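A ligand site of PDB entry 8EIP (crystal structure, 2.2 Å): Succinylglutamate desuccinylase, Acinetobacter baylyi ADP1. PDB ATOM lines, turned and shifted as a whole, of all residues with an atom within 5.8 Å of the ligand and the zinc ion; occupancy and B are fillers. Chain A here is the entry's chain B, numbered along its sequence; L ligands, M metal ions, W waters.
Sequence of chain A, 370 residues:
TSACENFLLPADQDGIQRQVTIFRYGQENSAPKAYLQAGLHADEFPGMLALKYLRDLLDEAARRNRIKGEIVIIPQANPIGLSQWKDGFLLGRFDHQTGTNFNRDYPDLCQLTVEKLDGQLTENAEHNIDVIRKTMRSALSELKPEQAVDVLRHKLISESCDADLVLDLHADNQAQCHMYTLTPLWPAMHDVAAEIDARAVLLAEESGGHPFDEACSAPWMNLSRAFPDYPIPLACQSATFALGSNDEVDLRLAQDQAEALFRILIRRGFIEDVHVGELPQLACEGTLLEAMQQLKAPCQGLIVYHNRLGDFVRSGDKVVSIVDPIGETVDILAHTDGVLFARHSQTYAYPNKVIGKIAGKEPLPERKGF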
ATOM      1  N   HIS A  41     -10.136  17.696  -7.471  1.00  0.00           N
ATOM      2  CA  HIS A  41      -9.186  18.819  -7.448  1.00  0.00           C
ATOM      3  C   HIS A  41      -9.433  19.348  -6.026  1.00  0.00           C
ATOM      4  O   HIS A  41     -10.545  19.804  -5.784  1.00  0.00           O
ATOM      5  CB  HIS A  41      -9.425  19.780  -8.604  1.00  0.00           C
ATOM      6  CG  HIS A  41      -8.945  19.293  -9.927  1.00  0.00           C
ATOM      7  ND1 HIS A  41      -9.705  19.395 -11.072  1.00  0.00           N
ATOM      8  CD2 HIS A  41      -7.783  18.704 -10.298  1.00  0.00           C
ATOM      9  CE1 HIS A  41      -9.036  18.885 -12.085  1.00  0.00           C
ATOM     10  NE2 HIS A  41      -7.863  18.460 -11.643  1.00  0.00           N
ATOM     11  N   GLU A  44     -11.108  22.810  -5.242  1.00  0.00           N
ATOM     12  CA  GLU A  44     -12.466  23.066  -5.796  1.00  0.00           C
ATOM     13  C   GLU A  44     -13.503  22.699  -4.725  1.00  0.00           C
ATOM     14  O   GLU A  44     -13.768  21.513  -4.540  1.00  0.00           O
ATOM     15  CB  GLU A  44     -12.623  22.305  -7.102  1.00  0.00           C
ATOM     16  CG  GLU A  44     -11.605  22.739  -8.131  1.00  0.00           C
ATOM     17  CD  GLU A  44     -11.755  22.108  -9.486  1.00  0.00           C
ATOM     18  OE1 GLU A  44     -12.634  21.230  -9.608  1.00  0.00           O
ATOM     19  OE2 GLU A  44     -10.966  22.458 -10.391  1.00  0.00           O
ATOM     20  N   ARG A  93      -4.567  20.927  -7.595  1.00  0.00           N
ATOM     21  CA  ARG A  93      -4.840  20.474  -8.982  1.00  0.00           C
ATOM     22  C   ARG A  93      -3.830  19.414  -9.424  1.00  0.00           C
ATOM     23  O   ARG A  93      -4.227  18.492 -10.158  1.00  0.00           O
ATOM     24  CB  ARG A  93      -4.782  21.675  -9.913  1.00  0.00           C
ATOM     25  CG  ARG A  93      -5.250  21.328 -11.309  1.00  0.00           C
ATOM     26  CD  ARG A  93      -5.430  22.607 -12.091  1.00  0.00           C
ATOM     27  NE  ARG A  93      -6.076  22.311 -13.357  1.00  0.00           N
ATOM     28  CZ  ARG A  93      -7.379  22.121 -13.510  1.00  0.00           C
ATOM     29  NH1 ARG A  93      -8.232  22.224 -12.495  1.00  0.00           N
ATOM     30  NH2 ARG A  93      -7.832  21.857 -14.724  1.00  0.00           N
ATOM     31  N   ASN A 101      -1.788  15.580 -13.086  1.00  0.00           N
ATOM     32  CA  ASN A 101      -3.105  16.192 -12.821  1.00  0.00           C
ATOM     33  C   ASN A 101      -3.971  15.126 -12.147  1.00  0.00           C
ATOM     34  O   ASN A 101      -4.071  13.997 -12.669  1.00  0.00           O
ATOM     35  CB  ASN A 101      -3.683  16.691 -14.120  1.00  0.00           C
ATOM     36  CG  ASN A 101      -4.958  17.479 -13.948  1.00  0.00           C
ATOM     37  OD1 ASN A 101      -5.902  17.024 -13.335  1.00  0.00           O
ATOM     38  ND2 ASN A 101      -5.010  18.598 -14.630  1.00  0.00           N
ATOM     39  N   ASN A 103      -7.104  14.806 -12.165  1.00  0.00           N
ATOM     40  CA  ASN A 103      -8.226  14.383 -13.030  1.00  0.00           C
ATOM     41  C   ASN A 103      -7.714  14.038 -14.422  1.00  0.00           C
ATOM     42  O   ASN A 103      -8.396  14.371 -15.406  1.00  0.00           O
ATOM     43  CB  ASN A 103      -9.348  15.401 -13.105  1.00  0.00           C
ATOM     44  CG  ASN A 103     -10.583  14.771 -13.696  1.00  0.00           C
ATOM     45  OD1 ASN A 103     -10.733  13.560 -13.643  1.00  0.00           O
ATOM     46  ND2 ASN A 103     -11.447  15.548 -14.317  1.00  0.00           N
ATOM     47  N   ARG A 104      -6.568  13.385 -14.497  1.00  0.00           N
ATOM     48  CA  ARG A 104      -6.035  12.848 -15.773  1.00  0.00           C
ATOM     49  C   ARG A 104      -5.447  11.464 -15.509  1.00  0.00           C
ATOM     50  O   ARG A 104      -5.309  11.081 -14.346  1.00  0.00           O
ATOM     51  CB  ARG A 104      -4.961  13.746 -16.380  1.00  0.00           C
ATOM     52  CG  ARG A 104      -5.415  15.157 -16.711  1.00  0.00           C
ATOM     53  CD  ARG A 104      -6.331  15.210 -17.899  1.00  0.00           C
ATOM     54  NE  ARG A 104      -6.621  16.590 -18.269  1.00  0.00           N
ATOM     55  CZ  ARG A 104      -7.566  17.360 -17.710  1.00  0.00           C
ATOM     56  NH1 ARG A 104      -8.364  16.888 -16.750  1.00  0.00           N
ATOM     57  NH2 ARG A 104      -7.728  18.605 -18.126  1.00  0.00           N
ATOM     58  N   ASP A 168     -19.315  13.623 -11.104  1.00  0.00           N
ATOM     59  CA  ASP A 168     -18.008  14.128 -10.624  1.00  0.00           C
ATOM     60  C   ASP A 168     -18.159  15.626 -10.367  1.00  0.00           C
ATOM     61  O   ASP A 168     -18.360  16.390 -11.334  1.00  0.00           O
ATOM     62  CB  ASP A 168     -16.925  13.796 -11.637  1.00  0.00           C
ATOM     63  CG  ASP A 168     -15.533  14.024 -11.082  1.00  0.00           C
ATOM     64  OD1 ASP A 168     -15.430  14.232  -9.839  1.00  0.00           O
ATOM     65  OD2 ASP A 168     -14.568  14.016 -11.874  1.00  0.00           O
ATOM     66  N   HIS A 170     -17.005  19.245  -9.502  1.00  0.00           N
ATOM     67  CA  HIS A 170     -15.830  20.112  -9.733  1.00  0.00           C
ATOM     68  C   HIS A 170     -16.231  21.584  -9.607  1.00  0.00           C
ATOM     69  O   HIS A 170     -17.395  21.896  -9.287  1.00  0.00           O
ATOM     70  CB  HIS A 170     -15.293  19.840 -11.138  1.00  0.00           C
ATOM     71  CG  HIS A 170     -14.497  18.593 -11.231  1.00  0.00           C
ATOM     72  ND1 HIS A 170     -13.113  18.601 -11.247  1.00  0.00           N
ATOM     73  CD2 HIS A 170     -14.865  17.311 -11.337  1.00  0.00           C
ATOM     74  CE1 HIS A 170     -12.669  17.370 -11.337  1.00  0.00           C
ATOM     75  NE2 HIS A 170     -13.725  16.555 -11.399  1.00  0.00           N
ATOM     76  N   ALA A 171     -15.263  22.446  -9.883  1.00  0.00           N
ATOM     77  CA  ALA A 171     -15.458  23.901  -9.993  1.00  0.00           C
ATOM     78  C   ALA A 171     -14.445  24.460 -10.982  1.00  0.00           C
ATOM     79  O   ALA A 171     -13.490  23.769 -11.335  1.00  0.00           O
ATOM     80  CB  ALA A 171     -15.350  24.508  -8.629  1.00  0.00           C
ATOM     81  N   ASP A 172     -14.643  25.692 -11.436  1.00  0.00           N
ATOM     82  CA  ASP A 172     -13.606  26.357 -12.249  1.00  0.00           C
ATOM     83  C   ASP A 172     -13.088  27.555 -11.464  1.00  0.00           C
ATOM     84  O   ASP A 172     -13.606  27.848 -10.402  1.00  0.00           O
ATOM     85  CB  ASP A 172     -14.148  26.727 -13.618  1.00  0.00           C
ATOM     86  CG  ASP A 172     -13.098  26.830 -14.693  1.00  0.00           C
ATOM     87  OD1 ASP A 172     -11.905  27.035 -14.354  1.00  0.00           O
ATOM     88  OD2 ASP A 172     -13.481  26.719 -15.879  1.00  0.00           O
ATOM     89  N   ASN A 173     -12.087  28.233 -11.971  1.00  0.00           N
ATOM     90  CA  ASN A 173     -11.446  29.281 -11.138  1.00  0.00           C
ATOM     91  C   ASN A 173     -12.424  30.423 -10.918  1.00  0.00           C
ATOM     92  O   ASN A 173     -12.497  30.944  -9.799  1.00  0.00           O
ATOM     93  CB  ASN A 173     -10.157  29.703 -11.772  1.00  0.00           C
ATOM     94  CG  ASN A 173      -9.139  28.611 -11.619  1.00  0.00           C
ATOM     95  OD1 ASN A 173      -8.826  27.904 -12.573  1.00  0.00           O
ATOM     96  ND2 ASN A 173      -8.613  28.467 -10.412  1.00  0.00           N
ATOM     97  N   TYR A 180     -20.065  18.896 -18.269  1.00  0.00           N
ATOM     98  CA  TYR A 180     -19.434  18.151 -19.379  1.00  0.00           C
ATOM     99  C   TYR A 180     -20.009  16.728 -19.412  1.00  0.00           C
ATOM    100  O   TYR A 180     -20.146  16.113 -18.346  1.00  0.00           O
ATOM    101  CB  TYR A 180     -17.929  17.994 -19.183  1.00  0.00           C
ATOM    102  CG  TYR A 180     -17.117  19.261 -19.079  1.00  0.00           C
ATOM    103  CD1 TYR A 180     -17.031  19.958 -17.892  1.00  0.00           C
ATOM    104  CD2 TYR A 180     -16.378  19.708 -20.168  1.00  0.00           C
ATOM    105  CE1 TYR A 180     -16.240  21.083 -17.786  1.00  0.00           C
ATOM    106  CE2 TYR A 180     -15.589  20.829 -20.075  1.00  0.00           C
ATOM    107  CZ  TYR A 180     -15.511  21.522 -18.886  1.00  0.00           C
ATOM    108  OH  TYR A 180     -14.744  22.621 -18.794  1.00  0.00           O
ATOM    109  N   ALA A 204     -18.046  15.905 -25.701  1.00  0.00           N
ATOM    110  CA  ALA A 204     -16.891  15.304 -26.406  1.00  0.00           C
ATOM    111  C   ALA A 204     -16.980  13.795 -26.337  1.00  0.00           C
ATOM    112  O   ALA A 204     -17.571  13.265 -25.389  1.00  0.00           O
ATOM    113  CB  ALA A 204     -15.599  15.816 -25.817  1.00  0.00           C
ATOM    114  N   SER A 207     -11.607  13.697 -24.809  1.00  0.00           N
ATOM    115  CA  SER A 207     -11.169  15.070 -24.461  1.00  0.00           C
ATOM    116  C   SER A 207      -9.649  15.102 -24.338  1.00  0.00           C
ATOM    117  O   SER A 207      -8.954  14.822 -25.312  1.00  0.00           O
ATOM    118  CB  SER A 207     -11.849  15.505 -23.222  1.00  0.00           C
ATOM    119  OG  SER A 207     -13.235  15.616 -23.428  1.00  0.00           O
ATOM    120  N   GLY A 208      -9.154  15.403 -23.152  1.00  0.00           N
ATOM    121  CA  GLY A 208      -7.723  15.407 -22.862  1.00  0.00           C
ATOM    122  C   GLY A 208      -7.252  14.040 -22.382  1.00  0.00           C
ATOM    123  O   GLY A 208      -7.865  13.021 -22.747  1.00  0.00           O
ATOM    124  N   PRO A 211      -9.630  11.875 -18.411  1.00  0.00           N
ATOM    125  CA  PRO A 211     -10.289  12.329 -17.185  1.00  0.00           C
ATOM    126  C   PRO A 211     -11.291  11.284 -16.639  1.00  0.00           C
ATOM    127  O   PRO A 211     -11.678  10.387 -17.366  1.00  0.00           O
ATOM    128  CB  PRO A 211     -10.996  13.615 -17.658  1.00  0.00           C
ATOM    129  CG  PRO A 211     -11.274  13.366 -19.113  1.00  0.00           C
ATOM    130  CD  PRO A 211     -10.054  12.618 -19.593  1.00  0.00           C
ATOM    131  N   ASP A 213     -14.602  11.310 -15.683  1.00  0.00           N
ATOM    132  CA  ASP A 213     -15.993  11.125 -16.169  1.00  0.00           C
ATOM    133  C   ASP A 213     -15.963  10.273 -17.455  1.00  0.00           C
ATOM    134  O   ASP A 213     -16.792   9.380 -17.598  1.00  0.00           O
ATOM    135  CB  ASP A 213     -16.678  12.461 -16.407  1.00  0.00           C
ATOM    136  CG  ASP A 213     -15.864  13.379 -17.289  1.00  0.00           C
ATOM    137  OD1 ASP A 213     -14.696  13.050 -17.583  1.00  0.00           O
ATOM    138  OD2 ASP A 213     -16.392  14.412 -17.684  1.00  0.00           O
ATOM    139  N   GLU A 214     -15.019  10.564 -18.346  1.00  0.00           N
ATOM    140  CA  GLU A 214     -14.874   9.808 -19.606  1.00  0.00           C
ATOM    141  C   GLU A 214     -14.391   8.395 -19.254  1.00  0.00           C
ATOM    142  O   GLU A 214     -14.851   7.454 -19.891  1.00  0.00           O
ATOM    143  CB  GLU A 214     -13.943  10.532 -20.582  1.00  0.00           C
ATOM    144  CG  GLU A 214     -14.561  11.797 -21.136  1.00  0.00           C
ATOM    145  CD  GLU A 214     -13.752  12.485 -22.227  1.00  0.00           C
ATOM    146  OE1 GLU A 214     -12.650  11.995 -22.555  1.00  0.00           O
ATOM    147  OE2 GLU A 214     -14.218  13.505 -22.747  1.00  0.00           O
ATOM    148  N   THR A 240     -19.525  15.602 -15.589  1.00  0.00           N
ATOM    149  CA  THR A 240     -18.767  16.490 -14.699  1.00  0.00           C
ATOM    150  C   THR A 240     -19.606  17.723 -14.468  1.00  0.00           C
ATOM    151  O   THR A 240     -20.020  18.368 -15.434  1.00  0.00           O
ATOM    152  CB  THR A 240     -17.402  16.880 -15.240  1.00  0.00           C
ATOM    153  OG1 THR A 240     -16.594  15.708 -15.340  1.00  0.00           O
ATOM    154  CG2 THR A 240     -16.729  17.882 -14.325  1.00  0.00           C
ATOM    155  N   ASN A 246     -14.088  28.004  -7.818  1.00  0.00           N
ATOM    156  CA  ASN A 246     -13.330  27.146  -6.876  1.00  0.00           C
ATOM    157  C   ASN A 246     -13.607  27.536  -5.423  1.00  0.00           C
ATOM    158  O   ASN A 246     -13.712  26.645  -4.572  1.00  0.00           O
ATOM    159  CB  ASN A 246     -11.834  27.256  -7.132  1.00  0.00           C
ATOM    160  CG  ASN A 246     -11.417  26.523  -8.385  1.00  0.00           C
ATOM    161  OD1 ASN A 246     -12.224  25.929  -9.078  1.00  0.00           O
ATOM    162  ND2 ASN A 246     -10.134  26.541  -8.676  1.00  0.00           N
ATOM    163  N   LEU A 289     -17.410  20.581 -27.276  1.00  0.00           N
ATOM    164  CA  LEU A 289     -16.245  21.134 -26.565  1.00  0.00           C
ATOM    165  C   LEU A 289     -15.344  21.811 -27.586  1.00  0.00           C
ATOM    166  O   LEU A 289     -14.800  22.863 -27.291  1.00  0.00           O
ATOM    167  CB  LEU A 289     -15.537  20.000 -25.832  1.00  0.00           C
ATOM    168  CG  LEU A 289     -14.399  20.452 -24.924  1.00  0.00           C
ATOM    169  CD1 LEU A 289     -14.892  21.441 -23.873  1.00  0.00           C
ATOM    170  CD2 LEU A 289     -13.725  19.273 -24.258  1.00  0.00           C
ATOM    171  N   VAL A 354      -5.043  30.155 -19.873  1.00  0.00           N
ATOM    172  CA  VAL A 354      -6.478  30.252 -20.233  1.00  0.00           C
ATOM    173  C   VAL A 354      -7.111  31.202 -19.229  1.00  0.00           C
ATOM    174  O   VAL A 354      -7.011  30.956 -18.027  1.00  0.00           O
ATOM    175  CB  VAL A 354      -7.156  28.881 -20.274  1.00  0.00           C
ATOM    176  CG1 VAL A 354      -8.645  29.035 -20.566  1.00  0.00           C
ATOM    177  CG2 VAL A 354      -6.469  28.024 -21.321  1.00  0.00           C
ATOM    178  N   LYS A 357     -13.604  31.327 -20.993  1.00  0.00           N
ATOM    179  CA  LYS A 357     -14.227  30.328 -21.884  1.00  0.00           C
ATOM    180  C   LYS A 357     -15.557  30.844 -22.421  1.00  0.00           C
ATOM    181  O   LYS A 357     -16.399  31.290 -21.621  1.00  0.00           O
ATOM    182  CB  LYS A 357     -14.465  29.019 -21.148  1.00  0.00           C
ATOM    183  CG  LYS A 357     -13.222  28.358 -20.589  1.00  0.00           C
ATOM    184  CD  LYS A 357     -13.569  27.072 -19.859  1.00  0.00           C
ATOM    185  CE  LYS A 357     -12.360  26.360 -19.321  1.00  0.00           C
ATOM    186  NZ  LYS A 357     -11.873  27.016 -18.089  1.00  0.00           N
HETATM  187  C1  LIG L   1     -10.296  23.988 -14.812  1.00  0.00           C
HETATM  188  N1  LIG L   1      -9.801  25.209 -14.126  1.00  0.00           N
HETATM  189  C2  LIG L   1     -11.619  23.510 -14.213  1.00  0.00           C
HETATM  190  C3  LIG L   1     -11.719  22.011 -14.109  1.00  0.00           C
HETATM  191  N2  LIG L   1     -11.833  21.354 -15.262  1.00  0.00           N
HETATM  192  C4  LIG L   1     -12.384  20.009 -15.354  1.00  0.00           C
HETATM  193  C5  LIG L   1     -11.387  18.973 -14.819  1.00  0.00           C
HETATM  194  O1  LIG L   1     -11.827  18.092 -14.074  1.00  0.00           O
HETATM  195  O2  LIG L   1     -10.201  19.095 -15.168  1.00  0.00           O
HETATM  196  C6  LIG L   1     -12.877  19.659 -16.762  1.00  0.00           C
HETATM  197  C7  LIG L   1     -13.517  18.282 -16.862  1.00  0.00           C
HETATM  198  C8  LIG L   1     -13.932  18.010 -18.295  1.00  0.00           C
HETATM  199  N3  LIG L   1     -13.901  16.600 -18.656  1.00  0.00           N
HETATM  200  C9  LIG L   1     -14.119  16.150 -19.886  1.00  0.00           C
HETATM  201  N4  LIG L   1     -14.327  14.862 -20.088  1.00  0.00           N
HETATM  202  N5  LIG L   1     -14.108  16.977 -20.905  1.00  0.00           N
HETATM  203  O3  LIG L   1     -11.709  21.434 -13.026  1.00  0.00           O
HETATM  204  C10 LIG L   1     -10.383  24.276 -16.320  1.00  0.00           C
HETATM  205  O4  LIG L   1      -9.661  25.175 -16.757  1.00  0.00           O
HETATM  206  O5  LIG L   1     -11.162  23.586 -16.989  1.00  0.00           O
HETATM  207 ZN    ZN M   1     -11.939  19.986 -11.601  1.00  0.00          ZN
HETATM  208  O   HOH W   1      -6.893  25.556 -13.390  1.00  0.00           O
HETATM  209  O   HOH W   2     -17.527  13.777 -19.716  1.00  0.00           O
HETATM  210  O   HOH W   3     -10.372  25.037 -11.267  1.00  0.00           O
HETATM  211  O   HOH W   4      -7.807  24.922 -18.727  1.00  0.00           O
HETATM  212  O   HOH W   5     -17.108  17.172 -22.542  1.00  0.00           O
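The side-chain amide nitrogen of Asn 103 is in hydrogen-bond range of an oxygen (O1) of the ligand, at 2.6 Å. OD1 of Asp 172 is in salt-bridge range of N1 of the ligand (2.8 Å). The side-chain carboxylate (OE2) of Glu 214 is in salt-bridge range of a nitrogen (N4) of the ligand (3.0 Å). N5 of the ligand is in hydrogen-bond range of OG of Ser 207, at 3.0 Å. OD1 of Asp 213 is in salt-bridge range of N4 of the ligand (3.1 Å). An oxygen (O4) of the ligand lies within salt-bridge range of the side-chain amino group of Lys 357, 3.2 Å away. O2 of the ligand is in salt-bridge range of NH2 of Arg 93 (3.7 Å). The side-chain amide oxygen (OD1) of Asn 173 is in hydrogen-bond range of a nitrogen (N1) of the ligand, at 3.3 Å. The guanidinium group of Arg 104 lies within salt-bridge range of an oxygen (O2) of the ligand, at 3.3 Å.
NE2 of His 170 sits at hydrogen-bond distance from OD2 of Asp 168 (2.7 Å). A ring nitrogen (ND1) of His 41 lies close to the guanidinium group of Arg 93. The side-chain carboxylate of Asp 172 is in salt-bridge range of the side-chain amino group of Lys 357, at 2.7 Å. N of Asn 246 is in hydrogen-bond range of O of Asp 172 (2.6 Å). The side-chain carboxylate (OD2) of Asp 213 lies within hydrogen-bond range of the side-chain hydroxyl (OG1) of Thr 240 (2.7 Å). ND2 of Asn 173 sits close to ND2 of Asn 246, at 3.0 Å. The side-chain amide oxygen (OD1) of Asn 246 sits close to the backbone carbonyl oxygen (O) of Ala 171 (3.4 Å). The backbone carbonyl oxygen (O) of Tyr 180 lies within hydrogen-bond range of the backbone NH (N) of Thr 240, 2.9 Å away.
An oxygen (O3) of the ligand lies close to the backbone carbonyl oxygen of Ala 171, at 3.4 Å. Merely in contact with the ligand: Tyr 180 (3.5 Å) and Pro 211 (3.5 Å). 15 residues have an atom within 4 Å of the ligand: His 41, Glu 44, Arg 93, Asn 103, Arg 104, His 170, Ala 171, Asp 172, Asn 173, Tyr 180, Ser 207, Pro 211, Asp 213, Glu 214 and Lys 357.
The zinc ion is bound by a ring nitrogen (ND1) of His 170 (1.8 Å), an oxygen (O3) of the ligand (2.0 Å), a ring nitrogen (ND1) of His 41 (2.4 Å) and the side-chain carboxylate of Glu 44 (2.5 Å).
Water W1 lies within hydrogen-bond range of a nitrogen (N1) of the ligand (3.0 Å), the side-chain amide oxygen (OD1) of Asn 173 (3.1 Å) and the guanidinium group (NE) of Arg 93 (3.3 Å). Water W2 bridges the side-chain carboxylate of Asp 213 and a nitrogen (N4) of the ligand.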
